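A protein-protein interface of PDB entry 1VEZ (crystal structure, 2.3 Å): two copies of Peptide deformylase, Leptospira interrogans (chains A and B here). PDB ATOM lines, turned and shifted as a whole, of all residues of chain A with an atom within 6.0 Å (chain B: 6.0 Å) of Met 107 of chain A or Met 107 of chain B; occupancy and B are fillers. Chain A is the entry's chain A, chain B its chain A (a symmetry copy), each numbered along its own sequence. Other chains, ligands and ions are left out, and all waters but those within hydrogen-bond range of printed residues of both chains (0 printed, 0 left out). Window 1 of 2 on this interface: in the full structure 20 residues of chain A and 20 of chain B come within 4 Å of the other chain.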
ATOM      1  N   MET A   8      15.636 -12.193 -19.074  1.00  0.00           N
ATOM      2  CA  MET A   8      15.346 -11.010 -19.860  1.00  0.00           C
ATOM      3  C   MET A   8      16.059 -11.225 -21.191  1.00  0.00           C
ATOM      4  O   MET A   8      17.222 -11.633 -21.225  1.00  0.00           O
ATOM      5  CB  MET A   8      15.886  -9.772 -19.154  1.00  0.00           C
ATOM      6  CG  MET A   8      15.607  -8.478 -19.878  1.00  0.00           C
ATOM      7  SD  MET A   8      15.992  -7.095 -18.831  1.00  0.00           S
ATOM      8  CE  MET A   8      17.750  -7.265 -18.656  1.00  0.00           C
ATOM      9  N   GLU A  99      14.711  -3.354  -6.337  1.00  0.00           N
ATOM     10  CA  GLU A  99      14.131  -4.592  -6.833  1.00  0.00           C
ATOM     11  C   GLU A  99      15.069  -5.526  -7.590  1.00  0.00           C
ATOM     12  O   GLU A  99      16.084  -5.115  -8.171  1.00  0.00           O
ATOM     13  CB  GLU A  99      12.926  -4.281  -7.722  1.00  0.00           C
ATOM     14  CG  GLU A  99      11.690  -3.829  -6.972  1.00  0.00           C
ATOM     15  CD  GLU A  99      10.522  -3.552  -7.902  1.00  0.00           C
ATOM     16  OE1 GLU A  99      10.253  -4.383  -8.798  1.00  0.00           O
ATOM     17  OE2 GLU A  99       9.867  -2.507  -7.729  1.00  0.00           O
ATOM     18  N   GLY A 100      14.697  -6.797  -7.570  1.00  0.00           N
ATOM     19  CA  GLY A 100      15.430  -7.828  -8.271  1.00  0.00           C
ATOM     20  C   GLY A 100      14.354  -8.608  -9.003  1.00  0.00           C
ATOM     21  O   GLY A 100      13.163  -8.329  -8.845  1.00  0.00           O
ATOM     22  N   CYS A 101      14.747  -9.578  -9.806  1.00  0.00           N
ATOM     23  CA  CYS A 101      13.769 -10.361 -10.539  1.00  0.00           C
ATOM     24  C   CYS A 101      14.424 -11.662 -10.939  1.00  0.00           C
ATOM     25  O   CYS A 101      15.559 -11.668 -11.409  1.00  0.00           O
ATOM     26  CB  CYS A 101      13.306  -9.604 -11.783  1.00  0.00           C
ATOM     27  SG  CYS A 101      12.237 -10.571 -12.883  1.00  0.00           S
ATOM     28  N   VAL A 104      15.988 -11.590 -14.186  1.00  0.00           N
ATOM     29  CA  VAL A 104      17.108 -10.677 -14.389  1.00  0.00           C
ATOM     30  C   VAL A 104      18.104 -11.028 -13.285  1.00  0.00           C
ATOM     31  O   VAL A 104      18.396 -10.218 -12.409  1.00  0.00           O
ATOM     32  CB  VAL A 104      16.673  -9.200 -14.239  1.00  0.00           C
ATOM     33  CG1 VAL A 104      17.839  -8.269 -14.552  1.00  0.00           C
ATOM     34  CG2 VAL A 104      15.513  -8.906 -15.165  1.00  0.00           C
ATOM     35  N   PRO A 105      18.636 -12.257 -13.322  1.00  0.00           N
ATOM     36  CA  PRO A 105      19.594 -12.748 -12.331  1.00  0.00           C
ATOM     37  C   PRO A 105      20.858 -11.927 -12.120  1.00  0.00           C
ATOM     38  O   PRO A 105      21.449 -11.417 -13.072  1.00  0.00           O
ATOM     39  CB  PRO A 105      19.895 -14.167 -12.811  1.00  0.00           C
ATOM     40  CG  PRO A 105      19.732 -14.058 -14.290  1.00  0.00           C
ATOM     41  CD  PRO A 105      18.493 -13.217 -14.430  1.00  0.00           C
ATOM     42  N   GLY A 106      21.248 -11.804 -10.855  1.00  0.00           N
ATOM     43  CA  GLY A 106      22.454 -11.092 -10.481  1.00  0.00           C
ATOM     44  C   GLY A 106      22.386  -9.585 -10.405  1.00  0.00           C
ATOM     45  O   GLY A 106      23.407  -8.935 -10.190  1.00  0.00           O
ATOM     46  N   MET A 107      21.197  -9.014 -10.551  1.00  0.00           N
ATOM     47  CA  MET A 107      21.089  -7.562 -10.528  1.00  0.00           C
ATOM     48  C   MET A 107      20.011  -6.992  -9.616  1.00  0.00           C
ATOM     49  O   MET A 107      19.128  -7.706  -9.147  1.00  0.00           O
ATOM     50  CB  MET A 107      20.868  -7.061 -11.957  1.00  0.00           C
ATOM     51  CG  MET A 107      21.861  -7.642 -12.966  1.00  0.00           C
ATOM     52  SD  MET A 107      21.601  -6.995 -14.623  1.00  0.00           S
ATOM     53  CE  MET A 107      22.445  -5.433 -14.471  1.00  0.00           C
ATOM     54  N   ARG A 108      20.109  -5.692  -9.369  1.00  0.00           N
ATOM     55  CA  ARG A 108      19.149  -4.966  -8.550  1.00  0.00           C
ATOM     56  C   ARG A 108      19.040  -3.573  -9.137  1.00  0.00           C
ATOM     57  O   ARG A 108      20.030  -3.016  -9.615  1.00  0.00           O
ATOM     58  CB  ARG A 108      19.606  -4.869  -7.087  1.00  0.00           C
ATOM     59  CG  ARG A 108      19.596  -6.185  -6.339  1.00  0.00           C
ATOM     60  CD  ARG A 108      18.209  -6.784  -6.322  1.00  0.00           C
ATOM     61  NE  ARG A 108      18.243  -8.220  -6.067  1.00  0.00           N
ATOM     62  CZ  ARG A 108      18.412  -8.769  -4.872  1.00  0.00           C
ATOM     63  NH1 ARG A 108      18.558  -7.991  -3.805  1.00  0.00           N
ATOM     64  NH2 ARG A 108      18.440 -10.093  -4.744  1.00  0.00           N
ATOM     65  N   GLY A 109      17.834  -3.020  -9.106  1.00  0.00           N
ATOM     66  CA  GLY A 109      17.609  -1.693  -9.631  1.00  0.00           C
ATOM     67  C   GLY A 109      16.621  -0.972  -8.746  1.00  0.00           C
ATOM     68  O   GLY A 109      15.667  -1.572  -8.267  1.00  0.00           O
ATOM     69  N   TYR A 153      11.016  -4.986 -14.305  1.00  0.00           N
ATOM     70  CA  TYR A 153      11.366  -3.833 -13.490  1.00  0.00           C
ATOM     71  C   TYR A 153      12.405  -2.912 -14.128  1.00  0.00           C
ATOM     72  O   TYR A 153      12.479  -1.736 -13.782  1.00  0.00           O
ATOM     73  CB  TYR A 153      11.823  -4.278 -12.093  1.00  0.00           C
ATOM     74  CG  TYR A 153      13.266  -4.703 -11.989  1.00  0.00           C
ATOM     75  CD1 TYR A 153      14.273  -3.772 -11.714  1.00  0.00           C
ATOM     76  CD2 TYR A 153      13.627  -6.039 -12.143  1.00  0.00           C
ATOM     77  CE1 TYR A 153      15.616  -4.172 -11.594  1.00  0.00           C
ATOM     78  CE2 TYR A 153      14.952  -6.450 -12.025  1.00  0.00           C
ATOM     79  CZ  TYR A 153      15.940  -5.513 -11.748  1.00  0.00           C
ATOM     80  OH  TYR A 153      17.238  -5.930 -11.597  1.00  0.00           O
ATOM     81  N   PHE A 163      21.364   1.095 -10.760  1.00  0.00           N
ATOM     82  CA  PHE A 163      21.135  -0.217 -11.335  1.00  0.00           C
ATOM     83  C   PHE A 163      22.501  -0.897 -11.422  1.00  0.00           C
ATOM     84  O   PHE A 163      23.492  -0.254 -11.774  1.00  0.00           O
ATOM     85  CB  PHE A 163      20.508   0.000 -12.721  1.00  0.00           C
ATOM     86  CG  PHE A 163      20.226  -1.257 -13.483  1.00  0.00           C
ATOM     87  CD1 PHE A 163      19.665  -2.365 -12.859  1.00  0.00           C
ATOM     88  CD2 PHE A 163      20.469  -1.309 -14.854  1.00  0.00           C
ATOM     89  CE1 PHE A 163      19.346  -3.502 -13.590  1.00  0.00           C
ATOM     90  CE2 PHE A 163      20.149  -2.444 -15.590  1.00  0.00           C
ATOM     91  CZ  PHE A 163      19.587  -3.541 -14.957  1.00  0.00           C
ATOM     92  N   GLY A 164      22.572  -2.178 -11.083  1.00  0.00           N
ATOM     93  CA  GLY A 164      23.852  -2.853 -11.148  1.00  0.00           C
ATOM     94  C   GLY A 164      23.844  -4.296 -10.695  1.00  0.00           C
ATOM     95  O   GLY A 164      22.791  -4.867 -10.420  1.00  0.00           O
ATOM     96  N   PHE A 165      25.032  -4.888 -10.627  1.00  0.00           N
ATOM     97  CA  PHE A 165      25.181  -6.267 -10.201  1.00  0.00           C
ATOM     98  C   PHE A 165      25.273  -6.344  -8.681  1.00  0.00           C
ATOM     99  O   PHE A 165      25.952  -5.531  -8.043  1.00  0.00           O
ATOM    100  CB  PHE A 165      26.420  -6.887 -10.852  1.00  0.00           C
ATOM    101  CG  PHE A 165      26.347  -6.925 -12.349  1.00  0.00           C
ATOM    102  CD1 PHE A 165      26.670  -5.800 -13.100  1.00  0.00           C
ATOM    103  CD2 PHE A 165      25.890  -8.060 -13.004  1.00  0.00           C
ATOM    104  CE1 PHE A 165      26.534  -5.804 -14.483  1.00  0.00           C
ATOM    105  CE2 PHE A 165      25.748  -8.074 -14.383  1.00  0.00           C
ATOM    106  CZ  PHE A 165      26.070  -6.945 -15.127  1.00  0.00           C
ATOM    107  N   ASN A 166      24.569  -7.328  -8.122  1.00  0.00           N
ATOM    108  CA  ASN A 166      24.494  -7.571  -6.682  1.00  0.00           C
ATOM    109  C   ASN A 166      25.771  -7.418  -5.882  1.00  0.00           C
ATOM    110  O   ASN A 166      25.866  -6.548  -5.018  1.00  0.00           O
ATOM    111  CB  ASN A 166      23.946  -8.971  -6.426  1.00  0.00           C
ATOM    112  CG  ASN A 166      22.532  -9.132  -6.907  1.00  0.00           C
ATOM    113  OD1 ASN A 166      22.016 -10.244  -6.977  1.00  0.00           O
ATOM    114  ND2 ASN A 166      21.889  -8.019  -7.242  1.00  0.00           N
ATOM    115  N   LEU A 169      26.955  -3.852  -5.915  1.00  0.00           N
ATOM    116  CA  LEU A 169      26.098  -2.932  -5.186  1.00  0.00           C
ATOM    117  C   LEU A 169      26.281  -3.159  -3.695  1.00  0.00           C
ATOM    118  O   LEU A 169      26.305  -2.209  -2.915  1.00  0.00           O
ATOM    119  CB  LEU A 169      24.633  -3.154  -5.563  1.00  0.00           C
ATOM    120  CG  LEU A 169      24.211  -2.726  -6.968  1.00  0.00           C
ATOM    121  CD1 LEU A 169      22.814  -3.215  -7.248  1.00  0.00           C
ATOM    122  CD2 LEU A 169      24.291  -1.212  -7.094  1.00  0.00           C
ATOM    123  N   MET B   8      28.974  -2.703 -13.448  1.00  0.00           N
ATOM    124  CA  MET B   8      27.954  -1.688 -13.264  1.00  0.00           C
ATOM    125  C   MET B   8      27.470  -1.859 -11.827  1.00  0.00           C
ATOM    126  O   MET B   8      27.217  -2.978 -11.376  1.00  0.00           O
ATOM    127  CB  MET B   8      26.812  -1.916 -14.246  1.00  0.00           C
ATOM    128  CG  MET B   8      25.708  -0.891 -14.158  1.00  0.00           C
ATOM    129  SD  MET B   8      24.601  -1.062 -15.537  1.00  0.00           S
ATOM    130  CE  MET B   8      23.898  -2.662 -15.227  1.00  0.00           C
ATOM    131  N   GLU B  99      24.981  -3.290 -28.445  1.00  0.00           N
ATOM    132  CA  GLU B  99      26.191  -3.110 -27.660  1.00  0.00           C
ATOM    133  C   GLU B  99      26.325  -3.974 -26.410  1.00  0.00           C
ATOM    134  O   GLU B  99      25.339  -4.433 -25.816  1.00  0.00           O
ATOM    135  CB  GLU B  99      26.336  -1.642 -27.258  1.00  0.00           C
ATOM    136  CG  GLU B  99      26.753  -0.719 -28.385  1.00  0.00           C
ATOM    137  CD  GLU B  99      26.897   0.721 -27.926  1.00  0.00           C
ATOM    138  OE1 GLU B  99      27.520   0.958 -26.867  1.00  0.00           O
ATOM    139  OE2 GLU B  99      26.396   1.617 -28.630  1.00  0.00           O
ATOM    140  N   GLY B 100      27.576  -4.178 -26.026  1.00  0.00           N
ATOM    141  CA  GLY B 100      27.905  -4.931 -24.836  1.00  0.00           C
ATOM    142  C   GLY B 100      28.930  -4.065 -24.128  1.00  0.00           C
ATOM    143  O   GLY B 100      29.334  -3.022 -24.648  1.00  0.00           O
ATOM    144  N   CYS B 101      29.358  -4.471 -22.948  1.00  0.00           N
ATOM    145  CA  CYS B 101      30.335  -3.688 -22.215  1.00  0.00           C
ATOM    146  C   CYS B 101      30.998  -4.598 -21.209  1.00  0.00           C
ATOM    147  O   CYS B 101      30.325  -5.366 -20.527  1.00  0.00           O
ATOM    148  CB  CYS B 101      29.653  -2.523 -21.498  1.00  0.00           C
ATOM    149  SG  CYS B 101      30.746  -1.596 -20.387  1.00  0.00           S
ATOM    150  N   VAL B 104      29.410  -4.629 -17.974  1.00  0.00           N
ATOM    151  CA  VAL B 104      28.039  -5.121 -17.886  1.00  0.00           C
ATOM    152  C   VAL B 104      28.082  -6.513 -18.512  1.00  0.00           C
ATOM    153  O   VAL B 104      27.460  -6.770 -19.541  1.00  0.00           O
ATOM    154  CB  VAL B 104      27.061  -4.227 -18.685  1.00  0.00           C
ATOM    155  CG1 VAL B 104      25.627  -4.708 -18.496  1.00  0.00           C
ATOM    156  CG2 VAL B 104      27.188  -2.788 -18.234  1.00  0.00           C
ATOM    157  N   PRO B 105      28.830  -7.432 -17.887  1.00  0.00           N
ATOM    158  CA  PRO B 105      28.984  -8.806 -18.367  1.00  0.00           C
ATOM    159  C   PRO B 105      27.711  -9.613 -18.581  1.00  0.00           C
ATOM    160  O   PRO B 105      26.771  -9.538 -17.790  1.00  0.00           O
ATOM    161  CB  PRO B 105      29.905  -9.439 -17.325  1.00  0.00           C
ATOM    162  CG  PRO B 105      29.558  -8.692 -16.080  1.00  0.00           C
ATOM    163  CD  PRO B 105      29.449  -7.272 -16.559  1.00  0.00           C
ATOM    164  N   GLY B 106      27.701 -10.374 -19.673  1.00  0.00           N
ATOM    165  CA  GLY B 106      26.586 -11.239 -20.004  1.00  0.00           C
ATOM    166  C   GLY B 106      25.382 -10.610 -20.665  1.00  0.00           C
ATOM    167  O   GLY B 106      24.376 -11.285 -20.874  1.00  0.00           O
ATOM    168  N   MET B 107      25.472  -9.336 -21.025  1.00  0.00           N
ATOM    169  CA  MET B 107      24.320  -8.677 -21.626  1.00  0.00           C
ATOM    170  C   MET B 107      24.597  -7.901 -22.907  1.00  0.00           C
ATOM    171  O   MET B 107      25.743  -7.629 -23.255  1.00  0.00           O
ATOM    172  CB  MET B 107      23.687  -7.746 -20.589  1.00  0.00           C
ATOM    173  CG  MET B 107      23.442  -8.418 -19.237  1.00  0.00           C
ATOM    174  SD  MET B 107      22.655  -7.309 -18.061  1.00  0.00           S
ATOM    175  CE  MET B 107      20.964  -7.448 -18.603  1.00  0.00           C
ATOM    176  N   ARG B 108      23.521  -7.559 -23.604  1.00  0.00           N
ATOM    177  CA  ARG B 108      23.586  -6.783 -24.834  1.00  0.00           C
ATOM    178  C   ARG B 108      22.345  -5.913 -24.867  1.00  0.00           C
ATOM    179  O   ARG B 108      21.274  -6.333 -24.427  1.00  0.00           O
ATOM    180  CB  ARG B 108      23.609  -7.686 -26.076  1.00  0.00           C
ATOM    181  CG  ARG B 108      24.881  -8.489 -26.244  1.00  0.00           C
ATOM    182  CD  ARG B 108      26.083  -7.578 -26.346  1.00  0.00           C
ATOM    183  NE  ARG B 108      27.320  -8.276 -26.016  1.00  0.00           N
ATOM    184  CZ  ARG B 108      27.965  -9.093 -26.837  1.00  0.00           C
ATOM    185  NH1 ARG B 108      27.488  -9.314 -28.057  1.00  0.00           N
ATOM    186  NH2 ARG B 108      29.084  -9.693 -26.438  1.00  0.00           N
ATOM    187  N   GLY B 109      22.498  -4.699 -25.382  1.00  0.00           N
ATOM    188  CA  GLY B 109      21.386  -3.782 -25.472  1.00  0.00           C
ATOM    189  C   GLY B 109      21.484  -3.011 -26.766  1.00  0.00           C
ATOM    190  O   GLY B 109      22.574  -2.638 -27.182  1.00  0.00           O
ATOM    191  N   TYR B 153      26.381   2.191 -21.532  1.00  0.00           N
ATOM    192  CA  TYR B 153      25.430   2.047 -22.624  1.00  0.00           C
ATOM    193  C   TYR B 153      23.995   1.792 -22.168  1.00  0.00           C
ATOM    194  O   TYR B 153      23.056   2.067 -22.911  1.00  0.00           O
ATOM    195  CB  TYR B 153      25.890   0.953 -23.600  1.00  0.00           C
ATOM    196  CG  TYR B 153      25.542  -0.459 -23.200  1.00  0.00           C
ATOM    197  CD1 TYR B 153      24.322  -1.032 -23.573  1.00  0.00           C
ATOM    198  CD2 TYR B 153      26.439  -1.232 -22.467  1.00  0.00           C
ATOM    199  CE1 TYR B 153      24.007  -2.356 -23.220  1.00  0.00           C
ATOM    200  CE2 TYR B 153      26.142  -2.545 -22.114  1.00  0.00           C
ATOM    201  CZ  TYR B 153      24.926  -3.102 -22.495  1.00  0.00           C
ATOM    202  OH  TYR B 153      24.655  -4.407 -22.174  1.00  0.00           O
ATOM    203  N   PHE B 163      16.914  -5.368 -24.672  1.00  0.00           N
ATOM    204  CA  PHE B 163      17.991  -5.480 -23.707  1.00  0.00           C
ATOM    205  C   PHE B 163      17.851  -6.856 -23.057  1.00  0.00           C
ATOM    206  O   PHE B 163      16.737  -7.290 -22.762  1.00  0.00           O
ATOM    207  CB  PHE B 163      17.811  -4.340 -22.693  1.00  0.00           C
ATOM    208  CG  PHE B 163      18.826  -4.313 -21.594  1.00  0.00           C
ATOM    209  CD1 PHE B 163      20.173  -4.526 -21.855  1.00  0.00           C
ATOM    210  CD2 PHE B 163      18.434  -4.011 -20.291  1.00  0.00           C
ATOM    211  CE1 PHE B 163      21.115  -4.434 -20.839  1.00  0.00           C
ATOM    212  CE2 PHE B 163      19.372  -3.915 -19.271  1.00  0.00           C
ATOM    213  CZ  PHE B 163      20.714  -4.126 -19.545  1.00  0.00           C
ATOM    214  N   GLY B 164      18.960  -7.555 -22.854  1.00  0.00           N
ATOM    215  CA  GLY B 164      18.863  -8.865 -22.244  1.00  0.00           C
ATOM    216  C   GLY B 164      20.174  -9.608 -22.099  1.00  0.00           C
ATOM    217  O   GLY B 164      21.243  -9.063 -22.367  1.00  0.00           O
ATOM    218  N   PHE B 165      20.085 -10.859 -21.662  1.00  0.00           N
ATOM    219  CA  PHE B 165      21.256 -11.696 -21.481  1.00  0.00           C
ATOM    220  C   PHE B 165      21.622 -12.386 -22.790  1.00  0.00           C
ATOM    221  O   PHE B 165      20.748 -12.872 -23.519  1.00  0.00           O
ATOM    222  CB  PHE B 165      21.001 -12.726 -20.377  1.00  0.00           C
ATOM    223  CG  PHE B 165      20.727 -12.107 -19.040  1.00  0.00           C
ATOM    224  CD1 PHE B 165      19.456 -11.640 -18.725  1.00  0.00           C
ATOM    225  CD2 PHE B 165      21.754 -11.927 -18.124  1.00  0.00           C
ATOM    226  CE1 PHE B 165      19.212 -10.999 -17.517  1.00  0.00           C
ATOM    227  CE2 PHE B 165      21.522 -11.287 -16.915  1.00  0.00           C
ATOM    228  CZ  PHE B 165      20.249 -10.820 -16.609  1.00  0.00           C
ATOM    229  N   ASN B 166      22.924 -12.405 -23.074  1.00  0.00           N
ATOM    230  CA  ASN B 166      23.492 -12.991 -24.287  1.00  0.00           C
ATOM    231  C   ASN B 166      22.904 -14.301 -24.770  1.00  0.00           C
ATOM    232  O   ASN B 166      22.329 -14.365 -25.855  1.00  0.00           O
ATOM    233  CB  ASN B 166      24.993 -13.190 -24.106  1.00  0.00           C
ATOM    234  CG  ASN B 166      25.729 -11.892 -23.936  1.00  0.00           C
ATOM    235  OD1 ASN B 166      26.899 -11.879 -23.565  1.00  0.00           O
ATOM    236  ND2 ASN B 166      25.050 -10.784 -24.209  1.00  0.00           N
ATOM    237  N   LEU B 169      19.330 -13.855 -25.837  1.00  0.00           N
ATOM    238  CA  LEU B 169      19.160 -13.053 -27.037  1.00  0.00           C
ATOM    239  C   LEU B 169      19.598 -13.867 -28.244  1.00  0.00           C
ATOM    240  O   LEU B 169      18.972 -13.808 -29.300  1.00  0.00           O
ATOM    241  CB  LEU B 169      19.997 -11.776 -26.950  1.00  0.00           C
ATOM    242  CG  LEU B 169      19.532 -10.716 -25.953  1.00  0.00           C
ATOM    243  CD1 LEU B 169      20.577  -9.640 -25.833  1.00  0.00           C
ATOM    244  CD2 LEU B 169      18.201 -10.131 -26.402  1.00  0.00           C
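Met 8 of chain A touches Gly 164 of chain B, and with the chains exchanged Gly 164 of chain A touches Met 8 of chain B.
Met 8 of chain A touches Phe 165 of chain B, and with the chains exchanged Phe 165 of chain A touches Met 8 of chain B.
Val 104 of chain A touches Phe 165 of chain B, and with the chains exchanged Phe 165 of chain A touches Val 104 of chain B.
Met 107 of chain A touches its own counterpart, Met 107 of chain B.
Tyr 153 of chain A touches none of the printed residues of chain B.
Printed residues of chain B within 4 Å of Phe 163 of chain A: Met 8 (3.3 Å).
Of the printed residues of chain B, Gly 164 of chain A touches Met 8 (3.4 Å).
Printed residues of chain A within 4 Å of Met 8 of chain B: Met 107 (3.2 Å), Phe 163 (3.3 Å), Gly 164 (3.4 Å) and Phe 165 (3.0 Å).
Printed residues of chain A within 4 Å of Val 104 of chain B: Phe 165.
Printed residues of chain A within 4 Å of Met 107 of chain B: Met 8 (3.2 Å) and Met 107 (3.6 Å).
Of the printed residues of chain A, Gly 164 of chain B touches Met 8.
The nearest residue of chain A that does not touch Met 107 of chain B is Phe 165 of chain A (4.5 Å).
O of Met 8 of chain A sits at hydrogen-bond distance from N of Phe 165 of chain B (3.0 Å).
The backbone carbonyl oxygen of Met 8 of chain B is in hydrogen-bond range of the backbone NH of Phe 165 of chain A (3.0 Å).
The side-chain sulfur (SD) of Met 107 of chain B sits close to the side-chain sulfur (SD) of Met 107 of chain A.
Among the printed residues, merely in contact across the chains: Met 107 of chain A with Met 8 of chain B (3.2 Å), Met 8 of chain A with Met 107 of chain B (3.2 Å), Phe 163 of chain A with Met 8 of chain B (3.3 Å), Met 8 of chain A with Phe 163 of chain B (3.3 Å), Gly 164 of chain A with Met 8 of chain B (3.4 Å), Met 8 of chain A with Gly 164 of chain B (3.4 Å), Phe 165 of chain A with Pro 105 of chain B (3.7 Å), Pro 105 of chain A with Phe 165 of chain B (3.7 Å), Phe 165 of chain A with Val 104 of chain B (3.8 Å) and Val 104 of chain A with Phe 165 of chain B (3.8 Å).
The side-chain amide nitrogen (ND2) of Asn 166 of chain A lies close to the backbone carbonyl oxygen (O) of Met 107 of chain A (3.4 Å).
The backbone NH (N) of Arg 108 of chain A lies within hydrogen-bond range of the backbone carbonyl oxygen (O) of Gly 164 of chain A, 3.0 Å away.
ND2 of Asn 166 of chain B lies close to O of Met 107 of chain B.
O of Gly 164 of chain B sits at hydrogen-bond distance from N of Arg 108 of chain B.
Printed residues of chain A that touch a printed residue of chain B: Met 8, Val 104, Pro 105, Met 107, Phe 163, Gly 164 and Phe 165.
Hydrophobic or aromatic side chains of chain A that line the printed part of chain B: Met 8, Pro 105, Met 107, Phe 163 and Phe 165.
Of the 16 printed residues of chain B, 7 touch a printed residue of chain A.
Among the printed residues, no Asp or Glu carboxylate lies within 4 Å of a Lys or Arg side-chain nitrogen of the other chain.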
